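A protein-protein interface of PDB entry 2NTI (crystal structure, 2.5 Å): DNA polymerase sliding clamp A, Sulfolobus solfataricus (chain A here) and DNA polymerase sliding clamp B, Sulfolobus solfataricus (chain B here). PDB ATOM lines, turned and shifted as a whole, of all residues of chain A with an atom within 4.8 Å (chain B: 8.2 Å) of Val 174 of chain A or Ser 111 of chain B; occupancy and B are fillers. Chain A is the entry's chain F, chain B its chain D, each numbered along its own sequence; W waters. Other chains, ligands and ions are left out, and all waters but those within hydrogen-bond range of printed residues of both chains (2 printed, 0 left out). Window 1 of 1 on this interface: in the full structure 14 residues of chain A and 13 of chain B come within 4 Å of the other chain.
The backbone carbonyl oxygen of Glu 173 of chain A sits close to the backbone carbonyl oxygen of Lys 110 of chain B (3.2 Å).
The side-chain carboxylate of Glu 145 of chain A is in hydrogen-bond range of the side-chain hydroxyl of Ser 111 of chain B, at 3.0 Å.
The backbone carbonyl oxygen of Lys 110 of chain B sits at hydrogen-bond distance from the backbone NH of Glu 175 of chain A, at 2.8 Å.
N of Thr 112 of chain B sits at hydrogen-bond distance from O of Glu 173 of chain A, 2.8 Å away.
The backbone carbonyl oxygen of Ala 109 of chain B sits at hydrogen-bond distance from the backbone NH of Asp 104 of chain B, 2.8 Å away.
O of Ile 164 of chain A sits at hydrogen-bond distance from N of Val 174 of chain A (2.8 Å).
The backbone carbonyl oxygen of Ile 162 of chain A sits at hydrogen-bond distance from the backbone NH of Phe 176 of chain A (3.1 Å).
The backbone carbonyl oxygen (O) of Ser 111 of chain B lies within hydrogen-bond range of the backbone NH (N) of Ile 102 of chain B (2.7 Å).
Among the printed residues, pairs that only touch across the chains: Val 174 of chain A with Lys 110 of chain B (3.2 Å), Val 172 of chain A with Thr 112 of chain B (3.4 Å), Glu 145 of chain A with Ile 78 of chain B (3.4 Å), Glu 173 of chain A with Ser 111 of chain B (3.5 Å), Glu 145 of chain A with Ala 82 of chain B (3.5 Å), Phe 176 of chain A with Ala 109 of chain B (3.5 Å), Glu 175 of chain A with Ala 109 of chain B (3.6 Å), Val 172 of chain A with Ile 78 of chain B (3.7 Å), Glu 175 of chain A with Gly 108 of chain B (3.7 Å), Val 174 of chain A with Ser 111 of chain B (3.7 Å), Glu 145 of chain A with Lys 81 of chain B (3.7 Å) and Val 174 of chain A with Ala 109 of chain B (3.97 Å).
Printed residues of chain B within 4 Å of Glu 145 of chain A: Ile 78, Lys 81, Ala 82 and Ser 111.
Val 174 of chain A touches just these residues of chain B: Ala 109, Lys 110 and Ser 111.
Printed residues of chain B within 4 Å of Glu 175 of chain A: Gly 108 (3.7 Å), Ala 109 (3.6 Å) and Lys 110 (2.8 Å).
Of the printed residues of chain A, Lys 81 of chain B touches Glu 145.
Printed residues of chain A within 4 Å of Ala 82 of chain B: Glu 145.
Of the printed residues of chain A, Gly 108 of chain B touches Glu 175.
Hydrophobic or aromatic side chains of chain A that line the printed part of chain B: Val 172, Val 174 and Phe 176.
Along chain A the printed residues that touch a printed residue of chain B span positions 145 to 176.
Of the 22 printed residues of chain B, 8 touch a printed residue of chain A.
Hydrophobic or aromatic side chains of chain B within 4 Å of the printed part of chain A: Ile 78, Ala 82 and Ala 109.
Among the printed residues, 16 pairs touch across the chains.
Water W1 lies within hydrogen-bond range of the side-chain hydroxyl (OG1) of Thr 112 of chain B (2.6 Å), the backbone carbonyl oxygen (O) of Lys 110 of chain B (2.8 Å) and the backbone carbonyl oxygen (O) of Glu 173 of chain A (3.0 Å).
Water W2 lies within hydrogen-bond range of O of Ala 82 of chain B and OE1 of Glu 145 of chain A.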
ATOM      1  N   ALA A 142      10.550 -18.893  -4.380  1.00  0.00           N
ATOM      2  CA  ALA A 142      10.583 -20.328  -4.100  1.00  0.00           C
ATOM      3  C   ALA A 142       9.559 -20.722  -3.044  1.00  0.00           C
ATOM      4  O   ALA A 142       8.888 -21.728  -3.182  1.00  0.00           O
ATOM      5  CB  ALA A 142      11.974 -20.764  -3.686  1.00  0.00           C
ATOM      6  N   GLU A 145       5.949 -20.354  -4.550  1.00  0.00           N
ATOM      7  CA  GLU A 145       5.655 -21.429  -5.491  1.00  0.00           C
ATOM      8  C   GLU A 145       5.315 -22.730  -4.779  1.00  0.00           C
ATOM      9  O   GLU A 145       4.324 -23.375  -5.094  1.00  0.00           O
ATOM     10  CB  GLU A 145       6.837 -21.657  -6.436  1.00  0.00           C
ATOM     11  CG  GLU A 145       7.056 -20.558  -7.458  1.00  0.00           C
ATOM     12  CD  GLU A 145       8.466 -20.567  -8.025  1.00  0.00           C
ATOM     13  OE1 GLU A 145       8.991 -19.465  -8.334  1.00  0.00           O
ATOM     14  OE2 GLU A 145       9.055 -21.668  -8.158  1.00  0.00           O
ATOM     15  N   VAL A 146       6.147 -23.102  -3.817  1.00  0.00           N
ATOM     16  CA  VAL A 146       6.006 -24.364  -3.113  1.00  0.00           C
ATOM     17  C   VAL A 146       4.754 -24.370  -2.232  1.00  0.00           C
ATOM     18  O   VAL A 146       4.067 -25.387  -2.132  1.00  0.00           O
ATOM     19  CB  VAL A 146       7.316 -24.696  -2.348  1.00  0.00           C
ATOM     20  CG1 VAL A 146       7.068 -25.538  -1.117  1.00  0.00           C
ATOM     21  CG2 VAL A 146       8.305 -25.375  -3.284  1.00  0.00           C
ATOM     22  N   ILE A 162      21.487 -25.627  -2.492  1.00  0.00           N
ATOM     23  CA  ILE A 162      20.379 -25.727  -1.555  1.00  0.00           C
ATOM     24  C   ILE A 162      19.092 -25.889  -2.364  1.00  0.00           C
ATOM     25  O   ILE A 162      18.966 -25.336  -3.456  1.00  0.00           O
ATOM     26  CB  ILE A 162      20.292 -24.495  -0.621  1.00  0.00           C
ATOM     27  CG1 ILE A 162      19.208 -24.699   0.435  1.00  0.00           C
ATOM     28  CG2 ILE A 162      20.080 -23.194  -1.416  1.00  0.00           C
ATOM     29  CD1 ILE A 162      18.886 -23.454   1.261  1.00  0.00           C
ATOM     30  N   LEU A 163      18.144 -26.658  -1.835  1.00  0.00           N
ATOM     31  CA  LEU A 163      16.889 -26.925  -2.535  1.00  0.00           C
ATOM     32  C   LEU A 163      15.674 -26.658  -1.665  1.00  0.00           C
ATOM     33  O   LEU A 163      15.633 -27.062  -0.506  1.00  0.00           O
ATOM     34  CB  LEU A 163      16.820 -28.384  -3.029  1.00  0.00           C
ATOM     35  CG  LEU A 163      18.004 -29.091  -3.717  1.00  0.00           C
ATOM     36  CD1 LEU A 163      17.657 -30.540  -4.009  1.00  0.00           C
ATOM     37  CD2 LEU A 163      18.421 -28.384  -4.991  1.00  0.00           C
ATOM     38  N   ILE A 164      14.684 -25.988  -2.250  1.00  0.00           N
ATOM     39  CA  ILE A 164      13.405 -25.745  -1.611  1.00  0.00           C
ATOM     40  C   ILE A 164      12.330 -26.525  -2.376  1.00  0.00           C
ATOM     41  O   ILE A 164      12.168 -26.350  -3.580  1.00  0.00           O
ATOM     42  CB  ILE A 164      13.088 -24.236  -1.542  1.00  0.00           C
ATOM     43  CG1 ILE A 164      14.274 -23.469  -0.931  1.00  0.00           C
ATOM     44  CG2 ILE A 164      11.806 -23.998  -0.757  1.00  0.00           C
ATOM     45  CD1 ILE A 164      14.035 -22.005  -0.690  1.00  0.00           C
ATOM     46  N   VAL A 172       7.512 -30.354  -6.715  1.00  0.00           N
ATOM     47  CA  VAL A 172       8.160 -29.129  -7.149  1.00  0.00           C
ATOM     48  C   VAL A 172       9.478 -29.022  -6.422  1.00  0.00           C
ATOM     49  O   VAL A 172       9.575 -29.345  -5.241  1.00  0.00           O
ATOM     50  CB  VAL A 172       7.318 -27.877  -6.815  1.00  0.00           C
ATOM     51  CG1 VAL A 172       7.866 -26.644  -7.545  1.00  0.00           C
ATOM     52  CG2 VAL A 172       5.846 -28.109  -7.146  1.00  0.00           C
ATOM     53  N   GLU A 173      10.494 -28.567  -7.135  1.00  0.00           N
ATOM     54  CA  GLU A 173      11.774 -28.317  -6.514  1.00  0.00           C
ATOM     55  C   GLU A 173      12.492 -27.126  -7.123  1.00  0.00           C
ATOM     56  O   GLU A 173      12.645 -27.008  -8.340  1.00  0.00           O
ATOM     57  CB  GLU A 173      12.630 -29.588  -6.436  1.00  0.00           C
ATOM     58  CG  GLU A 173      13.298 -30.043  -7.714  1.00  0.00           C
ATOM     59  CD  GLU A 173      14.438 -30.995  -7.388  1.00  0.00           C
ATOM     60  OE1 GLU A 173      14.146 -32.183  -7.089  1.00  0.00           O
ATOM     61  OE2 GLU A 173      15.616 -30.552  -7.417  1.00  0.00           O
ATOM     62  N   VAL A 174      12.883 -26.211  -6.251  1.00  0.00           N
ATOM     63  CA  VAL A 174      13.551 -24.997  -6.664  1.00  0.00           C
ATOM     64  C   VAL A 174      14.999 -25.084  -6.191  1.00  0.00           C
ATOM     65  O   VAL A 174      15.258 -25.220  -5.000  1.00  0.00           O
ATOM     66  CB  VAL A 174      12.847 -23.735  -6.103  1.00  0.00           C
ATOM     67  CG1 VAL A 174      13.462 -22.483  -6.679  1.00  0.00           C
ATOM     68  CG2 VAL A 174      11.363 -23.770  -6.413  1.00  0.00           C
ATOM     69  N   GLU A 175      15.931 -25.019  -7.138  1.00  0.00           N
ATOM     70  CA  GLU A 175      17.356 -25.174  -6.854  1.00  0.00           C
ATOM     71  C   GLU A 175      18.145 -23.876  -6.972  1.00  0.00           C
ATOM     72  O   GLU A 175      17.957 -23.099  -7.903  1.00  0.00           O
ATOM     73  CB  GLU A 175      17.968 -26.225  -7.788  1.00  0.00           C
ATOM     74  CG  GLU A 175      19.488 -26.354  -7.698  1.00  0.00           C
ATOM     75  CD  GLU A 175      20.047 -27.406  -8.627  1.00  0.00           C
ATOM     76  OE1 GLU A 175      19.610 -28.577  -8.547  1.00  0.00           O
ATOM     77  OE2 GLU A 175      20.942 -27.059  -9.426  1.00  0.00           O
ATOM     78  N   PHE A 176      19.038 -23.663  -6.016  1.00  0.00           N
ATOM     79  CA  PHE A 176      20.003 -22.576  -6.083  1.00  0.00           C
ATOM     80  C   PHE A 176      21.369 -23.216  -5.944  1.00  0.00           C
ATOM     81  O   PHE A 176      21.720 -23.722  -4.876  1.00  0.00           O
ATOM     82  CB  PHE A 176      19.763 -21.565  -4.966  1.00  0.00           C
ATOM     83  CG  PHE A 176      18.375 -20.982  -4.955  1.00  0.00           C
ATOM     84  CD1 PHE A 176      18.103 -19.783  -5.616  1.00  0.00           C
ATOM     85  CD2 PHE A 176      17.339 -21.622  -4.269  1.00  0.00           C
ATOM     86  CE1 PHE A 176      16.816 -19.231  -5.598  1.00  0.00           C
ATOM     87  CE2 PHE A 176      16.052 -21.086  -4.251  1.00  0.00           C
ATOM     88  CZ  PHE A 176      15.788 -19.890  -4.914  1.00  0.00           C
ATOM     89  N   ILE B  78       1.899 -22.089  -9.783  1.00  0.00           N
ATOM     90  CA  ILE B  78       3.366 -22.110  -9.719  1.00  0.00           C
ATOM     91  C   ILE B  78       3.974 -21.532 -10.995  1.00  0.00           C
ATOM     92  O   ILE B  78       4.859 -20.677 -10.937  1.00  0.00           O
ATOM     93  CB  ILE B  78       3.921 -23.548  -9.517  1.00  0.00           C
ATOM     94  CG1 ILE B  78       3.335 -24.189  -8.256  1.00  0.00           C
ATOM     95  CG2 ILE B  78       5.454 -23.546  -9.468  1.00  0.00           C
ATOM     96  CD1 ILE B  78       3.314 -25.706  -8.284  1.00  0.00           C
ATOM     97  N   LEU B  79       3.488 -22.015 -12.139  1.00  0.00           N
ATOM     98  CA  LEU B  79       3.949 -21.577 -13.445  1.00  0.00           C
ATOM     99  C   LEU B  79       3.800 -20.072 -13.604  1.00  0.00           C
ATOM    100  O   LEU B  79       4.685 -19.407 -14.142  1.00  0.00           O
ATOM    101  CB  LEU B  79       3.177 -22.306 -14.545  1.00  0.00           C
ATOM    102  CG  LEU B  79       3.494 -23.794 -14.697  1.00  0.00           C
ATOM    103  CD1 LEU B  79       2.363 -24.528 -15.393  1.00  0.00           C
ATOM    104  CD2 LEU B  79       4.796 -23.976 -15.446  1.00  0.00           C
ATOM    105  N   LYS B  81       3.773 -17.680 -11.198  1.00  0.00           N
ATOM    106  CA  LYS B  81       4.754 -16.919 -10.436  1.00  0.00           C
ATOM    107  C   LYS B  81       6.209 -17.170 -10.830  1.00  0.00           C
ATOM    108  O   LYS B  81       7.032 -16.266 -10.720  1.00  0.00           O
ATOM    109  CB  LYS B  81       4.554 -17.043  -8.925  1.00  0.00           C
ATOM    110  CG  LYS B  81       4.189 -18.409  -8.415  1.00  0.00           C
ATOM    111  CD  LYS B  81       3.613 -18.301  -7.010  1.00  0.00           C
ATOM    112  CE  LYS B  81       2.399 -17.363  -6.972  1.00  0.00           C
ATOM    113  NZ  LYS B  81       1.932 -17.162  -5.576  1.00  0.00           N
ATOM    114  N   ALA B  82       6.513 -18.371 -11.315  1.00  0.00           N
ATOM    115  CA  ALA B  82       7.877 -18.718 -11.719  1.00  0.00           C
ATOM    116  C   ALA B  82       8.245 -18.204 -13.108  1.00  0.00           C
ATOM    117  O   ALA B  82       9.428 -18.068 -13.425  1.00  0.00           O
ATOM    118  CB  ALA B  82       8.105 -20.223 -11.636  1.00  0.00           C
ATOM    119  N   SER B  83       7.240 -17.915 -13.930  1.00  0.00           N
ATOM    120  CA  SER B  83       7.486 -17.472 -15.302  1.00  0.00           C
ATOM    121  C   SER B  83       7.921 -16.018 -15.359  1.00  0.00           C
ATOM    122  O   SER B  83       7.099 -15.112 -15.238  1.00  0.00           O
ATOM    123  CB  SER B  83       6.257 -17.708 -16.184  1.00  0.00           C
ATOM    124  OG  SER B  83       6.064 -19.100 -16.383  1.00  0.00           O
ATOM    125  N   THR B  88      13.840 -19.081 -19.060  1.00  0.00           N
ATOM    126  CA  THR B  88      13.566 -19.970 -20.177  1.00  0.00           C
ATOM    127  C   THR B  88      12.730 -21.130 -19.664  1.00  0.00           C
ATOM    128  O   THR B  88      12.746 -21.431 -18.471  1.00  0.00           O
ATOM    129  CB  THR B  88      14.850 -20.516 -20.842  1.00  0.00           C
ATOM    130  OG1 THR B  88      15.620 -21.243 -19.880  1.00  0.00           O
ATOM    131  CG2 THR B  88      15.693 -19.390 -21.419  1.00  0.00           C
ATOM    132  N   ILE B  89      11.994 -21.778 -20.558  1.00  0.00           N
ATOM    133  CA  ILE B  89      11.123 -22.874 -20.145  1.00  0.00           C
ATOM    134  C   ILE B  89      11.367 -24.164 -20.924  1.00  0.00           C
ATOM    135  O   ILE B  89      11.361 -24.178 -22.152  1.00  0.00           O
ATOM    136  CB  ILE B  89       9.623 -22.460 -20.136  1.00  0.00           C
ATOM    137  CG1 ILE B  89       8.746 -23.589 -19.565  1.00  0.00           C
ATOM    138  CG2 ILE B  89       9.179 -21.974 -21.514  1.00  0.00           C
ATOM    139  CD1 ILE B  89       7.387 -23.139 -19.044  1.00  0.00           C
ATOM    140  N   GLU B  90      11.604 -25.239 -20.180  1.00  0.00           N
ATOM    141  CA  GLU B  90      11.835 -26.550 -20.761  1.00  0.00           C
ATOM    142  C   GLU B  90      10.701 -27.501 -20.407  1.00  0.00           C
ATOM    143  O   GLU B  90      10.245 -27.545 -19.269  1.00  0.00           O
ATOM    144  CB  GLU B  90      13.179 -27.122 -20.308  1.00  0.00           C
ATOM    145  CG  GLU B  90      13.544 -28.454 -20.977  1.00  0.00           C
ATOM    146  CD  GLU B  90      14.680 -29.177 -20.277  1.00  0.00           C
ATOM    147  OE1 GLU B  90      14.807 -30.413 -20.475  1.00  0.00           O
ATOM    148  OE2 GLU B  90      15.445 -28.517 -19.522  1.00  0.00           O
ATOM    149  N   LYS B  99       7.889 -33.068 -17.275  1.00  0.00           N
ATOM    150  CA  LYS B  99       8.592 -32.207 -16.347  1.00  0.00           C
ATOM    151  C   LYS B  99       8.842 -30.848 -16.974  1.00  0.00           C
ATOM    152  O   LYS B  99       9.345 -30.738 -18.095  1.00  0.00           O
ATOM    153  CB  LYS B  99       9.882 -32.845 -15.807  1.00  0.00           C
ATOM    154  CG  LYS B  99      11.017 -32.992 -16.805  1.00  0.00           C
ATOM    155  CD  LYS B  99      12.366 -32.904 -16.121  1.00  0.00           C
ATOM    156  CE  LYS B  99      12.936 -34.270 -15.796  1.00  0.00           C
ATOM    157  NZ  LYS B  99      14.304 -34.142 -15.214  1.00  0.00           N
ATOM    158  N   ILE B 100       8.446 -29.815 -16.243  1.00  0.00           N
ATOM    159  CA  ILE B 100       8.630 -28.433 -16.653  1.00  0.00           C
ATOM    160  C   ILE B 100       9.774 -27.816 -15.857  1.00  0.00           C
ATOM    161  O   ILE B 100       9.758 -27.843 -14.631  1.00  0.00           O
ATOM    162  CB  ILE B 100       7.350 -27.608 -16.429  1.00  0.00           C
ATOM    163  CG1 ILE B 100       6.188 -28.212 -17.227  1.00  0.00           C
ATOM    164  CG2 ILE B 100       7.597 -26.137 -16.775  1.00  0.00           C
ATOM    165  CD1 ILE B 100       4.858 -27.500 -17.057  1.00  0.00           C
ATOM    166  N   ILE B 101      10.762 -27.265 -16.559  1.00  0.00           N
ATOM    167  CA  ILE B 101      11.950 -26.706 -15.927  1.00  0.00           C
ATOM    168  C   ILE B 101      12.085 -25.227 -16.247  1.00  0.00           C
ATOM    169  O   ILE B 101      12.254 -24.849 -17.400  1.00  0.00           O
ATOM    170  CB  ILE B 101      13.246 -27.455 -16.350  1.00  0.00           C
ATOM    171  CG1 ILE B 101      13.093 -28.969 -16.133  1.00  0.00           C
ATOM    172  CG2 ILE B 101      14.448 -26.924 -15.571  1.00  0.00           C
ATOM    173  CD1 ILE B 101      14.228 -29.800 -16.750  1.00  0.00           C
ATOM    174  N   ILE B 102      12.011 -24.393 -15.218  1.00  0.00           N
ATOM    175  CA  ILE B 102      12.166 -22.956 -15.406  1.00  0.00           C
ATOM    176  C   ILE B 102      13.489 -22.471 -14.813  1.00  0.00           C
ATOM    177  O   ILE B 102      13.779 -22.712 -13.646  1.00  0.00           O
ATOM    178  CB  ILE B 102      10.958 -22.168 -14.857  1.00  0.00           C
ATOM    179  CG1 ILE B 102       9.674 -22.631 -15.564  1.00  0.00           C
ATOM    180  CG2 ILE B 102      11.176 -20.675 -15.054  1.00  0.00           C
ATOM    181  CD1 ILE B 102       8.363 -22.300 -14.842  1.00  0.00           C
ATOM    182  N   ARG B 103      14.291 -21.811 -15.641  1.00  0.00           N
ATOM    183  CA  ARG B 103      15.600 -21.322 -15.240  1.00  0.00           C
ATOM    184  C   ARG B 103      15.611 -19.813 -15.238  1.00  0.00           C
ATOM    185  O   ARG B 103      15.694 -19.190 -16.294  1.00  0.00           O
ATOM    186  CB  ARG B 103      16.676 -21.836 -16.191  1.00  0.00           C
ATOM    187  CG  ARG B 103      16.926 -23.318 -16.084  1.00  0.00           C
ATOM    188  CD  ARG B 103      17.595 -23.810 -17.368  1.00  0.00           C
ATOM    189  NE  ARG B 103      17.449 -25.255 -17.487  1.00  0.00           N
ATOM    190  CZ  ARG B 103      18.463 -26.121 -17.382  1.00  0.00           C
ATOM    191  NH1 ARG B 103      19.707 -25.685 -17.169  1.00  0.00           N
ATOM    192  NH2 ARG B 103      18.229 -27.422 -17.500  1.00  0.00           N
ATOM    193  N   ASP B 104      15.519 -19.237 -14.043  1.00  0.00           N
ATOM    194  CA  ASP B 104      15.479 -17.793 -13.889  1.00  0.00           C
ATOM    195  C   ASP B 104      16.891 -17.241 -13.960  1.00  0.00           C
ATOM    196  O   ASP B 104      17.724 -17.549 -13.120  1.00  0.00           O
ATOM    197  CB  ASP B 104      14.808 -17.400 -12.570  1.00  0.00           C
ATOM    198  CG  ASP B 104      14.503 -15.910 -12.487  1.00  0.00           C
ATOM    199  OD1 ASP B 104      13.385 -15.552 -12.075  1.00  0.00           O
ATOM    200  OD2 ASP B 104      15.371 -15.086 -12.831  1.00  0.00           O
ATOM    201  N   SER B 107      17.258 -14.406 -10.729  1.00  0.00           N
ATOM    202  CA  SER B 107      17.386 -14.917  -9.362  1.00  0.00           C
ATOM    203  C   SER B 107      18.298 -16.144  -9.266  1.00  0.00           C
ATOM    204  O   SER B 107      18.690 -16.555  -8.168  1.00  0.00           O
ATOM    205  CB  SER B 107      16.009 -15.196  -8.738  1.00  0.00           C
ATOM    206  OG  SER B 107      15.233 -16.088  -9.518  1.00  0.00           O
ATOM    207  N   GLY B 108      18.638 -16.710 -10.422  1.00  0.00           N
ATOM    208  CA  GLY B 108      19.435 -17.927 -10.490  1.00  0.00           C
ATOM    209  C   GLY B 108      18.695 -19.160  -9.997  1.00  0.00           C
ATOM    210  O   GLY B 108      19.313 -20.180  -9.699  1.00  0.00           O
ATOM    211  N   ALA B 109      17.370 -19.066  -9.907  1.00  0.00           N
ATOM    212  CA  ALA B 109      16.544 -20.170  -9.420  1.00  0.00           C
ATOM    213  C   ALA B 109      16.192 -21.133 -10.538  1.00  0.00           C
ATOM    214  O   ALA B 109      15.860 -20.716 -11.650  1.00  0.00           O
ATOM    215  CB  ALA B 109      15.281 -19.643  -8.767  1.00  0.00           C
ATOM    216  N   LYS B 110      16.279 -22.424 -10.240  1.00  0.00           N
ATOM    217  CA  LYS B 110      15.836 -23.431 -11.177  1.00  0.00           C
ATOM    218  C   LYS B 110      14.642 -24.171 -10.599  1.00  0.00           C
ATOM    219  O   LYS B 110      14.773 -24.954  -9.652  1.00  0.00           O
ATOM    220  CB  LYS B 110      16.959 -24.388 -11.563  1.00  0.00           C
ATOM    221  CG  LYS B 110      16.693 -25.093 -12.878  1.00  0.00           C
ATOM    222  CD  LYS B 110      16.913 -26.593 -12.750  1.00  0.00           C
ATOM    223  CE  LYS B 110      18.360 -26.976 -13.020  1.00  0.00           C
ATOM    224  NZ  LYS B 110      18.573 -28.385 -12.492  1.00  0.00           N
ATOM    225  N   SER B 111      13.476 -23.893 -11.174  1.00  0.00           N
ATOM    226  CA  SER B 111      12.237 -24.494 -10.732  1.00  0.00           C
ATOM    227  C   SER B 111      11.874 -25.671 -11.622  1.00  0.00           C
ATOM    228  O   SER B 111      11.712 -25.516 -12.827  1.00  0.00           O
ATOM    229  CB  SER B 111      11.119 -23.460 -10.740  1.00  0.00           C
ATOM    230  OG  SER B 111      11.416 -22.405  -9.853  1.00  0.00           O
ATOM    231  N   THR B 112      11.756 -26.847 -11.017  1.00  0.00           N
ATOM    232  CA  THR B 112      11.382 -28.055 -11.732  1.00  0.00           C
ATOM    233  C   THR B 112      10.047 -28.534 -11.192  1.00  0.00           C
ATOM    234  O   THR B 112       9.898 -28.743  -9.997  1.00  0.00           O
ATOM    235  CB  THR B 112      12.457 -29.179 -11.588  1.00  0.00           C
ATOM    236  OG1 THR B 112      13.728 -28.694 -12.040  1.00  0.00           O
ATOM    237  CG2 THR B 112      12.094 -30.409 -12.412  1.00  0.00           C
ATOM    238  N   ILE B 113       9.081 -28.692 -12.091  1.00  0.00           N
ATOM    239  CA  ILE B 113       7.754 -29.192 -11.736  1.00  0.00           C
ATOM    240  C   ILE B 113       7.497 -30.529 -12.421  1.00  0.00           C
ATOM    241  O   ILE B 113       7.576 -30.630 -13.640  1.00  0.00           O
ATOM    242  CB  ILE B 113       6.627 -28.199 -12.126  1.00  0.00           C
ATOM    243  CG1 ILE B 113       6.828 -26.830 -11.468  1.00  0.00           C
ATOM    244  CG2 ILE B 113       5.269 -28.760 -11.757  1.00  0.00           C
ATOM    245  CD1 ILE B 113       7.504 -25.794 -12.368  1.00  0.00           C
ATOM    246  N   TYR B 114       7.201 -31.553 -11.633  1.00  0.00           N
ATOM    247  CA  TYR B 114       6.852 -32.853 -12.184  1.00  0.00           C
ATOM    248  C   TYR B 114       5.343 -33.011 -12.233  1.00  0.00           C
ATOM    249  O   TYR B 114       4.658 -32.789 -11.238  1.00  0.00           O
ATOM    250  CB  TYR B 114       7.460 -33.980 -11.363  1.00  0.00           C
ATOM    251  CG  TYR B 114       8.961 -34.048 -11.420  1.00  0.00           C
ATOM    252  CD1 TYR B 114       9.611 -34.565 -12.539  1.00  0.00           C
ATOM    253  CD2 TYR B 114       9.736 -33.606 -10.346  1.00  0.00           C
ATOM    254  CE1 TYR B 114      10.997 -34.635 -12.593  1.00  0.00           C
ATOM    255  CE2 TYR B 114      11.121 -33.671 -10.386  1.00  0.00           C
ATOM    256  CZ  TYR B 114      11.746 -34.190 -11.513  1.00  0.00           C
ATOM    257  OH  TYR B 114      13.120 -34.257 -11.559  1.00  0.00           O
HETATM  258  O   HOH W   1      15.043 -27.676  -9.978  1.00  0.00           O
HETATM  259  O   HOH W   2      11.168 -18.216 -10.737  1.00  0.00           O
